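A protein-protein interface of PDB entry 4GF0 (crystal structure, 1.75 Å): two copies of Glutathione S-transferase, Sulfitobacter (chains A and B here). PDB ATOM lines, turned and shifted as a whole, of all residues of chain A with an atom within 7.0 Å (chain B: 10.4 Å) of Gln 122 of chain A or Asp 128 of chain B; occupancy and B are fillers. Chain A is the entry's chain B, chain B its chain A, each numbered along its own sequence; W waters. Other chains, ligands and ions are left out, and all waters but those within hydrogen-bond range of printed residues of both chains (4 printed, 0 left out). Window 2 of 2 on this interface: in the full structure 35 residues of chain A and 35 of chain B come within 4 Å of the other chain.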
ATOM      1  N   TRP A 119      11.925   9.376  -5.852  1.00  0.00           N
ATOM      2  CA  TRP A 119      12.488   8.482  -6.852  1.00  0.00           C
ATOM      3  C   TRP A 119      11.486   7.608  -7.574  1.00  0.00           C
ATOM      4  O   TRP A 119      11.859   6.881  -8.496  1.00  0.00           O
ATOM      5  CB  TRP A 119      13.547   7.580  -6.219  1.00  0.00           C
ATOM      6  CG  TRP A 119      14.632   8.307  -5.502  1.00  0.00           C
ATOM      7  CD1 TRP A 119      15.684   8.976  -6.061  1.00  0.00           C
ATOM      8  CD2 TRP A 119      14.790   8.417  -4.082  1.00  0.00           C
ATOM      9  NE1 TRP A 119      16.486   9.500  -5.075  1.00  0.00           N
ATOM     10  CE2 TRP A 119      15.960   9.178  -3.853  1.00  0.00           C
ATOM     11  CE3 TRP A 119      14.053   7.957  -2.985  1.00  0.00           C
ATOM     12  CZ2 TRP A 119      16.419   9.480  -2.562  1.00  0.00           C
ATOM     13  CZ3 TRP A 119      14.505   8.253  -1.706  1.00  0.00           C
ATOM     14  CH2 TRP A 119      15.681   9.013  -1.505  1.00  0.00           C
ATOM     15  N   ALA A 120      10.227   7.652  -7.153  1.00  0.00           N
ATOM     16  CA  ALA A 120       9.198   6.828  -7.775  1.00  0.00           C
ATOM     17  C   ALA A 120       7.861   7.551  -7.745  1.00  0.00           C
ATOM     18  O   ALA A 120       7.690   8.509  -6.989  1.00  0.00           O
ATOM     19  CB  ALA A 120       9.092   5.480  -7.064  1.00  0.00           C
ATOM     20  N   LYS A 121       6.915   7.083  -8.556  1.00  0.00           N
ATOM     21  CA  LYS A 121       5.602   7.709  -8.643  1.00  0.00           C
ATOM     22  C   LYS A 121       4.448   6.797  -8.227  1.00  0.00           C
ATOM     23  O   LYS A 121       3.376   7.280  -7.869  1.00  0.00           O
ATOM     24  CB  LYS A 121       5.337   8.199 -10.073  1.00  0.00           C
ATOM     25  CG  LYS A 121       6.040   9.485 -10.456  1.00  0.00           C
ATOM     26  CD  LYS A 121       5.383  10.100 -11.690  1.00  0.00           C
ATOM     27  CE  LYS A 121       6.040  11.418 -12.057  1.00  0.00           C
ATOM     28  NZ  LYS A 121       6.190  12.295 -10.863  1.00  0.00           N
ATOM     29  N   GLN A 122       4.645   5.486  -8.308  1.00  0.00           N
ATOM     30  CA  GLN A 122       3.532   4.552  -8.117  1.00  0.00           C
ATOM     31  C   GLN A 122       3.364   4.092  -6.675  1.00  0.00           C
ATOM     32  O   GLN A 122       4.338   3.788  -5.999  1.00  0.00           O
ATOM     33  CB  GLN A 122       3.684   3.334  -9.032  1.00  0.00           C
ATOM     34  CG  GLN A 122       3.719   3.674 -10.504  1.00  0.00           C
ATOM     35  CD  GLN A 122       3.724   2.448 -11.390  1.00  0.00           C
ATOM     36  OE1 GLN A 122       4.351   1.434 -11.070  1.00  0.00           O
ATOM     37  NE2 GLN A 122       3.013   2.530 -12.511  1.00  0.00           N
ATOM     38  N   GLN A 123       2.116   4.003  -6.221  1.00  0.00           N
ATOM     39  CA  GLN A 123       1.849   3.661  -4.825  1.00  0.00           C
ATOM     40  C   GLN A 123       2.408   2.296  -4.459  1.00  0.00           C
ATOM     41  O   GLN A 123       2.867   2.080  -3.339  1.00  0.00           O
ATOM     42  CB  GLN A 123       0.346   3.697  -4.544  1.00  0.00           C
ATOM     43  CG  GLN A 123      -0.001   3.506  -3.082  1.00  0.00           C
ATOM     44  CD  GLN A 123      -1.463   3.752  -2.830  1.00  0.00           C
ATOM     45  OE1 GLN A 123      -2.116   4.446  -3.604  1.00  0.00           O
ATOM     46  NE2 GLN A 123      -1.994   3.166  -1.764  1.00  0.00           N
ATOM     47  N   SER A 124       2.389   1.386  -5.425  1.00  0.00           N
ATOM     48  CA  SER A 124       2.945   0.053  -5.236  1.00  0.00           C
ATOM     49  C   SER A 124       4.455   0.092  -5.017  1.00  0.00           C
ATOM     50  O   SER A 124       4.997  -0.742  -4.292  1.00  0.00           O
ATOM     51  CB  SER A 124       2.582  -0.858  -6.418  1.00  0.00           C
ATOM     52  OG  SER A 124       2.976  -0.282  -7.650  1.00  0.00           O
ATOM     53  N   SER A 125       5.138   1.052  -5.638  1.00  0.00           N
ATOM     54  CA  SER A 125       6.577   1.215  -5.424  1.00  0.00           C
ATOM     55  C   SER A 125       6.843   1.699  -4.006  1.00  0.00           C
ATOM     56  O   SER A 125       7.813   1.288  -3.368  1.00  0.00           O
ATOM     57  CB  SER A 125       7.181   2.200  -6.433  1.00  0.00           C
ATOM     58  OG  SER A 125       6.995   1.741  -7.760  1.00  0.00           O
ATOM     59  N   PHE A 126       5.981   2.575  -3.504  1.00  0.00           N
ATOM     60  CA  PHE A 126       6.164   3.101  -2.155  1.00  0.00           C
ATOM     61  C   PHE A 126       6.006   2.003  -1.095  1.00  0.00           C
ATOM     62  O   PHE A 126       6.744   1.980  -0.099  1.00  0.00           O
ATOM     63  CB  PHE A 126       5.187   4.248  -1.879  1.00  0.00           C
ATOM     64  CG  PHE A 126       5.325   5.411  -2.830  1.00  0.00           C
ATOM     65  CD1 PHE A 126       6.555   5.743  -3.380  1.00  0.00           C
ATOM     66  CD2 PHE A 126       4.218   6.179  -3.168  1.00  0.00           C
ATOM     67  CE1 PHE A 126       6.682   6.822  -4.255  1.00  0.00           C
ATOM     68  CE2 PHE A 126       4.334   7.258  -4.044  1.00  0.00           C
ATOM     69  CZ  PHE A 126       5.569   7.577  -4.587  1.00  0.00           C
ATOM     70  N   GLU A 127       5.047   1.104  -1.307  1.00  0.00           N
ATOM     71  CA  GLU A 127       4.839  -0.011  -0.386  1.00  0.00           C
ATOM     72  C   GLU A 127       6.064  -0.932  -0.382  1.00  0.00           C
ATOM     73  O   GLU A 127       6.537  -1.349   0.677  1.00  0.00           O
ATOM     74  CB  GLU A 127       3.561  -0.774  -0.745  1.00  0.00           C
ATOM     75  CG  GLU A 127       3.129  -1.801   0.287  1.00  0.00           C
ATOM     76  CD  GLU A 127       3.868  -3.110   0.129  1.00  0.00           C
ATOM     77  OE1 GLU A 127       4.156  -3.482  -1.028  1.00  0.00           O
ATOM     78  OE2 GLU A 127       4.171  -3.759   1.154  1.00  0.00           O
ATOM     79  N   MET A 129       9.191  -0.071  -1.185  1.00  0.00           N
ATOM     80  CA  MET A 129      10.246   0.654  -0.469  1.00  0.00           C
ATOM     81  C   MET A 129      10.084   0.574   1.046  1.00  0.00           C
ATOM     82  O   MET A 129      11.043   0.272   1.764  1.00  0.00           O
ATOM     83  CB  MET A 129      10.265   2.127  -0.884  1.00  0.00           C
ATOM     84  CG  MET A 129      10.797   2.401  -2.271  1.00  0.00           C
ATOM     85  SD  MET A 129      10.560   4.144  -2.650  1.00  0.00           S
ATOM     86  CE  MET A 129      11.248   4.241  -4.302  1.00  0.00           C
ATOM     87  N   ALA B 109      20.277   9.782  -7.248  1.00  0.00           N
ATOM     88  CA  ALA B 109      19.259   9.794  -8.297  1.00  0.00           C
ATOM     89  C   ALA B 109      19.670   8.907  -9.469  1.00  0.00           C
ATOM     90  O   ALA B 109      18.861   8.142  -9.996  1.00  0.00           O
ATOM     91  CB  ALA B 109      18.967  11.219  -8.777  1.00  0.00           C
ATOM     92  N   HIS B 112      19.356   5.025  -9.037  1.00  0.00           N
ATOM     93  CA  HIS B 112      18.033   4.413  -9.143  1.00  0.00           C
ATOM     94  C   HIS B 112      17.740   3.867 -10.538  1.00  0.00           C
ATOM     95  O   HIS B 112      16.733   3.179 -10.744  1.00  0.00           O
ATOM     96  CB  HIS B 112      16.939   5.387  -8.691  1.00  0.00           C
ATOM     97  CG  HIS B 112      16.841   5.528  -7.211  1.00  0.00           C
ATOM     98  ND1 HIS B 112      17.776   6.218  -6.453  1.00  0.00           N
ATOM     99  CD2 HIS B 112      15.942   5.036  -6.328  1.00  0.00           C
ATOM    100  CE1 HIS B 112      17.435   6.160  -5.182  1.00  0.00           C
ATOM    101  NE2 HIS B 112      16.321   5.449  -5.078  1.00  0.00           N
ATOM    102  N   LYS B 113      18.609   4.164 -11.498  1.00  0.00           N
ATOM    103  CA  LYS B 113      18.417   3.647 -12.850  1.00  0.00           C
ATOM    104  C   LYS B 113      18.694   2.151 -12.931  1.00  0.00           C
ATOM    105  O   LYS B 113      17.884   1.394 -13.479  1.00  0.00           O
ATOM    106  CB  LYS B 113      19.291   4.396 -13.864  1.00  0.00           C
ATOM    107  CG  LYS B 113      19.013   3.984 -15.308  1.00  0.00           C
ATOM    108  CD  LYS B 113      19.637   4.946 -16.313  1.00  0.00           C
ATOM    109  CE  LYS B 113      21.119   4.711 -16.490  1.00  0.00           C
ATOM    110  NZ  LYS B 113      21.674   5.566 -17.586  1.00  0.00           N
ATOM    111  N   MET B 114      19.838   1.732 -12.391  1.00  0.00           N
ATOM    112  CA  MET B 114      20.296   0.349 -12.500  1.00  0.00           C
ATOM    113  C   MET B 114      20.380  -0.411 -11.176  1.00  0.00           C
ATOM    114  O   MET B 114      20.468  -1.640 -11.176  1.00  0.00           O
ATOM    115  CB  MET B 114      21.675   0.300 -13.168  1.00  0.00           C
ATOM    116  CG  MET B 114      21.711   0.789 -14.605  1.00  0.00           C
ATOM    117  SD  MET B 114      20.630  -0.175 -15.686  1.00  0.00           S
ATOM    118  CE  MET B 114      21.412   0.094 -17.278  1.00  0.00           C
ATOM    119  N   GLY B 116      18.145  -0.189  -8.519  1.00  0.00           N
ATOM    120  CA  GLY B 116      16.885  -0.110  -7.802  1.00  0.00           C
ATOM    121  C   GLY B 116      16.743  -1.185  -6.738  1.00  0.00           C
ATOM    122  O   GLY B 116      16.064  -0.979  -5.730  1.00  0.00           O
ATOM    123  N   ALA B 120      14.350  -1.725  -3.174  1.00  0.00           N
ATOM    124  CA  ALA B 120      13.075  -2.355  -3.525  1.00  0.00           C
ATOM    125  C   ALA B 120      13.308  -3.764  -4.043  1.00  0.00           C
ATOM    126  O   ALA B 120      14.433  -4.122  -4.384  1.00  0.00           O
ATOM    127  CB  ALA B 120      12.329  -1.525  -4.573  1.00  0.00           C
ATOM    128  N   GLN B 122      10.512  -5.486  -6.087  1.00  0.00           N
ATOM    129  CA  GLN B 122       9.626  -5.789  -7.210  1.00  0.00           C
ATOM    130  C   GLN B 122      10.058  -5.172  -8.537  1.00  0.00           C
ATOM    131  O   GLN B 122      10.541  -4.035  -8.589  1.00  0.00           O
ATOM    132  CB  GLN B 122       8.184  -5.384  -6.885  1.00  0.00           C
ATOM    133  CG  GLN B 122       7.682  -5.947  -5.565  1.00  0.00           C
ATOM    134  CD  GLN B 122       7.760  -7.461  -5.513  1.00  0.00           C
ATOM    135  OE1 GLN B 122       7.582  -8.140  -6.528  1.00  0.00           O
ATOM    136  NE2 GLN B 122       8.026  -8.001  -4.327  1.00  0.00           N
ATOM    137  N   GLN B 123       9.846  -5.931  -9.611  1.00  0.00           N
ATOM    138  CA  GLN B 123      10.226  -5.512 -10.952  1.00  0.00           C
ATOM    139  C   GLN B 123       9.492  -4.239 -11.351  1.00  0.00           C
ATOM    140  O   GLN B 123      10.069  -3.343 -11.967  1.00  0.00           O
ATOM    141  CB  GLN B 123       9.924  -6.635 -11.951  1.00  0.00           C
ATOM    142  CG  GLN B 123      10.191  -6.282 -13.412  1.00  0.00           C
ATOM    143  CD  GLN B 123      11.637  -5.894 -13.678  1.00  0.00           C
ATOM    144  OE1 GLN B 123      12.555  -6.333 -12.981  1.00  0.00           O
ATOM    145  NE2 GLN B 123      11.845  -5.061 -14.696  1.00  0.00           N
ATOM    146  N   SER B 124       8.217  -4.171 -10.992  1.00  0.00           N
ATOM    147  CA  SER B 124       7.400  -3.001 -11.284  1.00  0.00           C
ATOM    148  C   SER B 124       7.981  -1.766 -10.586  1.00  0.00           C
ATOM    149  O   SER B 124       7.951  -0.664 -11.136  1.00  0.00           O
ATOM    150  CB  SER B 124       5.956  -3.232 -10.851  1.00  0.00           C
ATOM    151  OG  SER B 124       5.899  -3.497  -9.465  1.00  0.00           O
ATOM    152  N   SER B 125       8.508  -1.948  -9.376  1.00  0.00           N
ATOM    153  CA  SER B 125       9.157  -0.850  -8.662  1.00  0.00           C
ATOM    154  C   SER B 125      10.422  -0.405  -9.387  1.00  0.00           C
ATOM    155  O   SER B 125      10.724   0.788  -9.459  1.00  0.00           O
ATOM    156  CB  SER B 125       9.505  -1.254  -7.224  1.00  0.00           C
ATOM    157  OG  SER B 125       8.333  -1.580  -6.493  1.00  0.00           O
ATOM    158  N   PHE B 126      11.173  -1.364  -9.919  1.00  0.00           N
ATOM    159  CA  PHE B 126      12.390  -1.030 -10.646  1.00  0.00           C
ATOM    160  C   PHE B 126      12.057  -0.213 -11.888  1.00  0.00           C
ATOM    161  O   PHE B 126      12.775   0.736 -12.212  1.00  0.00           O
ATOM    162  CB  PHE B 126      13.160  -2.289 -11.054  1.00  0.00           C
ATOM    163  CG  PHE B 126      13.567  -3.162  -9.899  1.00  0.00           C
ATOM    164  CD1 PHE B 126      13.818  -2.615  -8.651  1.00  0.00           C
ATOM    165  CD2 PHE B 126      13.702  -4.535 -10.068  1.00  0.00           C
ATOM    166  CE1 PHE B 126      14.196  -3.423  -7.588  1.00  0.00           C
ATOM    167  CE2 PHE B 126      14.080  -5.346  -9.009  1.00  0.00           C
ATOM    168  CZ  PHE B 126      14.326  -4.790  -7.771  1.00  0.00           C
ATOM    169  N   GLU B 127      10.977  -0.585 -12.578  1.00  0.00           N
ATOM    170  CA  GLU B 127      10.589   0.082 -13.811  1.00  0.00           C
ATOM    171  C   GLU B 127      10.140   1.503 -13.523  1.00  0.00           C
ATOM    172  O   GLU B 127      10.455   2.429 -14.274  1.00  0.00           O
ATOM    173  CB  GLU B 127       9.477  -0.701 -14.530  1.00  0.00           C
ATOM    174  CG  GLU B 127       9.925  -2.068 -15.024  1.00  0.00           C
ATOM    175  CD  GLU B 127       8.777  -2.909 -15.544  1.00  0.00           C
ATOM    176  OE1 GLU B 127       7.614  -2.448 -15.486  1.00  0.00           O
ATOM    177  OE2 GLU B 127       9.041  -4.038 -16.010  1.00  0.00           O
ATOM    178  N   ASP B 128       9.387   1.653 -12.435  1.00  0.00           N
ATOM    179  CA  ASP B 128       8.914   2.949 -11.964  1.00  0.00           C
ATOM    180  C   ASP B 128      10.121   3.848 -11.678  1.00  0.00           C
ATOM    181  O   ASP B 128      10.218   4.960 -12.200  1.00  0.00           O
ATOM    182  CB  ASP B 128       8.081   2.752 -10.689  1.00  0.00           C
ATOM    183  CG  ASP B 128       7.477   4.041 -10.163  1.00  0.00           C
ATOM    184  OD1 ASP B 128       7.619   5.096 -10.816  1.00  0.00           O
ATOM    185  OD2 ASP B 128       6.839   3.992  -9.087  1.00  0.00           O
ATOM    186  N   MET B 129      11.047   3.355 -10.867  1.00  0.00           N
ATOM    187  CA  MET B 129      12.203   4.162 -10.469  1.00  0.00           C
ATOM    188  C   MET B 129      13.080   4.521 -11.671  1.00  0.00           C
ATOM    189  O   MET B 129      13.566   5.648 -11.797  1.00  0.00           O
ATOM    190  CB  MET B 129      13.023   3.443  -9.382  1.00  0.00           C
ATOM    191  CG  MET B 129      12.268   3.302  -8.047  1.00  0.00           C
ATOM    192  SD  MET B 129      13.231   2.510  -6.735  1.00  0.00           S
ATOM    193  CE  MET B 129      13.393   0.850  -7.403  1.00  0.00           C
ATOM    194  N   THR B 130      13.286   3.556 -12.556  1.00  0.00           N
ATOM    195  CA  THR B 130      14.082   3.787 -13.752  1.00  0.00           C
ATOM    196  C   THR B 130      13.470   4.894 -14.617  1.00  0.00           C
ATOM    197  O   THR B 130      14.184   5.755 -15.131  1.00  0.00           O
ATOM    198  CB  THR B 130      14.241   2.482 -14.546  1.00  0.00           C
ATOM    199  OG1 THR B 130      15.025   1.566 -13.765  1.00  0.00           O
ATOM    200  CG2 THR B 130      14.925   2.732 -15.887  1.00  0.00           C
ATOM    201  N   ALA B 131      12.144   4.896 -14.737  1.00  0.00           N
ATOM    202  CA  ALA B 131      11.451   5.869 -15.582  1.00  0.00           C
ATOM    203  C   ALA B 131      11.584   7.310 -15.081  1.00  0.00           C
ATOM    204  O   ALA B 131      11.439   8.256 -15.859  1.00  0.00           O
ATOM    205  CB  ALA B 131       9.980   5.488 -15.738  1.00  0.00           C
ATOM    206  N   GLN B 132      11.864   7.479 -13.789  1.00  0.00           N
ATOM    207  CA  GLN B 132      11.933   8.811 -13.199  1.00  0.00           C
ATOM    208  C   GLN B 132      13.309   9.454 -13.339  1.00  0.00           C
ATOM    209  O   GLN B 132      13.446  10.656 -13.120  1.00  0.00           O
ATOM    210  CB  GLN B 132      11.559   8.784 -11.713  1.00  0.00           C
ATOM    211  CG  GLN B 132      10.275   8.051 -11.391  1.00  0.00           C
ATOM    212  CD  GLN B 132       9.128   8.438 -12.301  1.00  0.00           C
ATOM    213  OE1 GLN B 132       8.932   9.613 -12.621  1.00  0.00           O
ATOM    214  NE2 GLN B 132       8.359   7.440 -12.728  1.00  0.00           N
ATOM    215  N   VAL B 133      14.312   8.661 -13.700  1.00  0.00           N
ATOM    216  CA  VAL B 133      15.701   9.143 -13.745  1.00  0.00           C
ATOM    217  C   VAL B 133      15.949  10.361 -14.656  1.00  0.00           C
ATOM    218  O   VAL B 133      16.701  11.264 -14.278  1.00  0.00           O
ATOM    219  CB  VAL B 133      16.706   7.993 -14.053  1.00  0.00           C
ATOM    220  CG1 VAL B 133      18.137   8.524 -14.198  1.00  0.00           C
ATOM    221  CG2 VAL B 133      16.669   6.953 -12.944  1.00  0.00           C
ATOM    222  N   PRO B 134      15.336  10.397 -15.857  1.00  0.00           N
ATOM    223  CA  PRO B 134      15.552  11.612 -16.652  1.00  0.00           C
ATOM    224  C   PRO B 134      15.021  12.850 -15.941  1.00  0.00           C
ATOM    225  O   PRO B 134      15.609  13.929 -16.046  1.00  0.00           O
ATOM    226  CB  PRO B 134      14.753  11.341 -17.926  1.00  0.00           C
ATOM    227  CG  PRO B 134      14.788   9.860 -18.063  1.00  0.00           C
ATOM    228  CD  PRO B 134      14.676   9.343 -16.652  1.00  0.00           C
ATOM    229  N   GLU B 135      13.937  12.697 -15.192  1.00  0.00           N
ATOM    230  CA  GLU B 135      13.379  13.832 -14.469  1.00  0.00           C
ATOM    231  C   GLU B 135      14.147  14.192 -13.195  1.00  0.00           C
ATOM    232  O   GLU B 135      14.363  15.374 -12.924  1.00  0.00           O
ATOM    233  CB  GLU B 135      11.893  13.621 -14.190  1.00  0.00           C
ATOM    234  CG  GLU B 135      11.074  13.624 -15.476  1.00  0.00           C
ATOM    235  CD  GLU B 135       9.620  13.297 -15.244  1.00  0.00           C
ATOM    236  OE1 GLU B 135       9.064  13.750 -14.220  1.00  0.00           O
ATOM    237  OE2 GLU B 135       9.032  12.585 -16.088  1.00  0.00           O
ATOM    238  N   THR B 136      14.574  13.194 -12.422  1.00  0.00           N
ATOM    239  CA  THR B 136      15.332  13.477 -11.205  1.00  0.00           C
ATOM    240  C   THR B 136      16.720  14.038 -11.522  1.00  0.00           C
ATOM    241  O   THR B 136      17.209  14.924 -10.822  1.00  0.00           O
ATOM    242  CB  THR B 136      15.466  12.247 -10.279  1.00  0.00           C
ATOM    243  OG1 THR B 136      16.151  11.195 -10.970  1.00  0.00           O
ATOM    244  CG2 THR B 136      14.099  11.765  -9.835  1.00  0.00           C
HETATM  245  O   HOH W   1       5.253  -0.231  -8.769  1.00  0.00           O
HETATM  246  O   HOH W   2      14.231   7.131  -9.647  1.00  0.00           O
HETATM  247  O   HOH W   3       6.109   0.568 -13.115  1.00  0.00           O
HETATM  248  O   HOH W   4       5.903  -2.232  -7.324  1.00  0.00           O
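The side-chain carboxylate of Asp 128 of chain B lies within hydrogen-bond range of the side-chain amide nitrogen of Gln 132 of chain B, 3.1 Å away. The backbone carbonyl oxygen (O) of Gln 132 of chain B is in hydrogen-bond range of the side-chain hydroxyl (OG1) of Thr 136 of chain B, 3.5 Å away.
Among the printed residues, merely in contact across the chains: Trp 119 of chain A with His 112 of chain B, Trp 119 of chain A with Met 129 of chain B, Trp 119 of chain A with Gln 132 of chain B, Ala 120 of chain A with Asp 128 of chain B, Ala 120 of chain A with Met 129 of chain B, Ala 120 of chain A with Gln 132 of chain B, Lys 121 of chain A with Gln 132 of chain B, Ser 125 of chain A with Ser 125 of chain B and Met 129 of chain A with Met 129 of chain B.
Water W4 lies within hydrogen-bond range of the side-chain hydroxyl of Ser 124 of chain B (2.5 Å), the side-chain hydroxyl of Ser 125 of chain B (2.6 Å) and the backbone carbonyl oxygen of Ser 124 of chain A (3.5 Å). Water W1 lies within hydrogen-bond range of the side-chain hydroxyl (OG) of Ser 124 of chain A (2.5 Å), the side-chain hydroxyl (OG) of Ser 125 of chain A (2.8 Å), the side-chain amide oxygen (OE1) of Gln 122 of chain A (3.0 Å) and the side-chain hydroxyl (OG) of Ser 124 of chain B (3.4 Å). Water W2 bridges the backbone carbonyl oxygen of Trp 119 of chain A (2.6 Å) and the backbone carbonyl oxygen of Met 129 of chain B (2.7 Å). Water W3 lies within hydrogen-bond range of the side-chain amide oxygen of Gln 122 of chain A (2.8 Å) and the backbone carbonyl oxygen of Ser 124 of chain B (3.0 Å).
Hydrophobic or aromatic side chains of chain A that line the printed part of chain B: Trp 119, Ala 120 and Met 129. Among the printed residues, no Asp or Glu carboxylate lies within 4 Å of a Lys or Arg side-chain nitrogen of the other chain.
N of Lys 121 of chain A is in hydrogen-bond range of OD1 of Asp 128 of chain B (3.1 Å). OD2 of Asp 128 of chain B sits at hydrogen-bond distance from N of Gln 122 of chain A (2.8 Å). OG of Ser 125 of chain A is in hydrogen-bond range of OD2 of Asp 128 of chain B, at 2.6 Å.
Ala 120 of chain A touches Met 129 of chain B, but with the chains exchanged Met 129 of chain A does not touch Ala 120 of chain B (4.8 Å). Ser 125 of chain B touches its own counterpart, Ser 125 of chain A. Met 129 of chain A touches its own counterpart, Met 129 of chain B. 8 positions are printed for both chains.
Of the printed residues of chain B, Gln 122 of chain A touches Asp 128 (2.8 Å). Of chain A, only Ala 120 (3.4 Å), Lys 121 (3.1 Å), Gln 122 (2.8 Å) and Ser 125 (2.6 Å) come within 4 Å of Asp 128 of chain B. No residue of chain B comes within 4 Å of Ser 124 of chain A. Of the printed residues of chain A, Ser 125 of chain B touches Ser 125. Of the printed residues of chain A, Met 129 of chain B touches Trp 119, Ala 120 and Met 129. Of the printed residues of chain B, Lys 121 of chain A touches Asp 128 and Gln 132. Of the printed residues of chain A, Gln 132 of chain B touches Trp 119 (3.5 Å), Ala 120 (3.97 Å) and Lys 121 (3.5 Å). Met 114 of chain B touches none of the printed residues of chain A. Gln 123 of chain B touches none of the printed residues of chain A.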
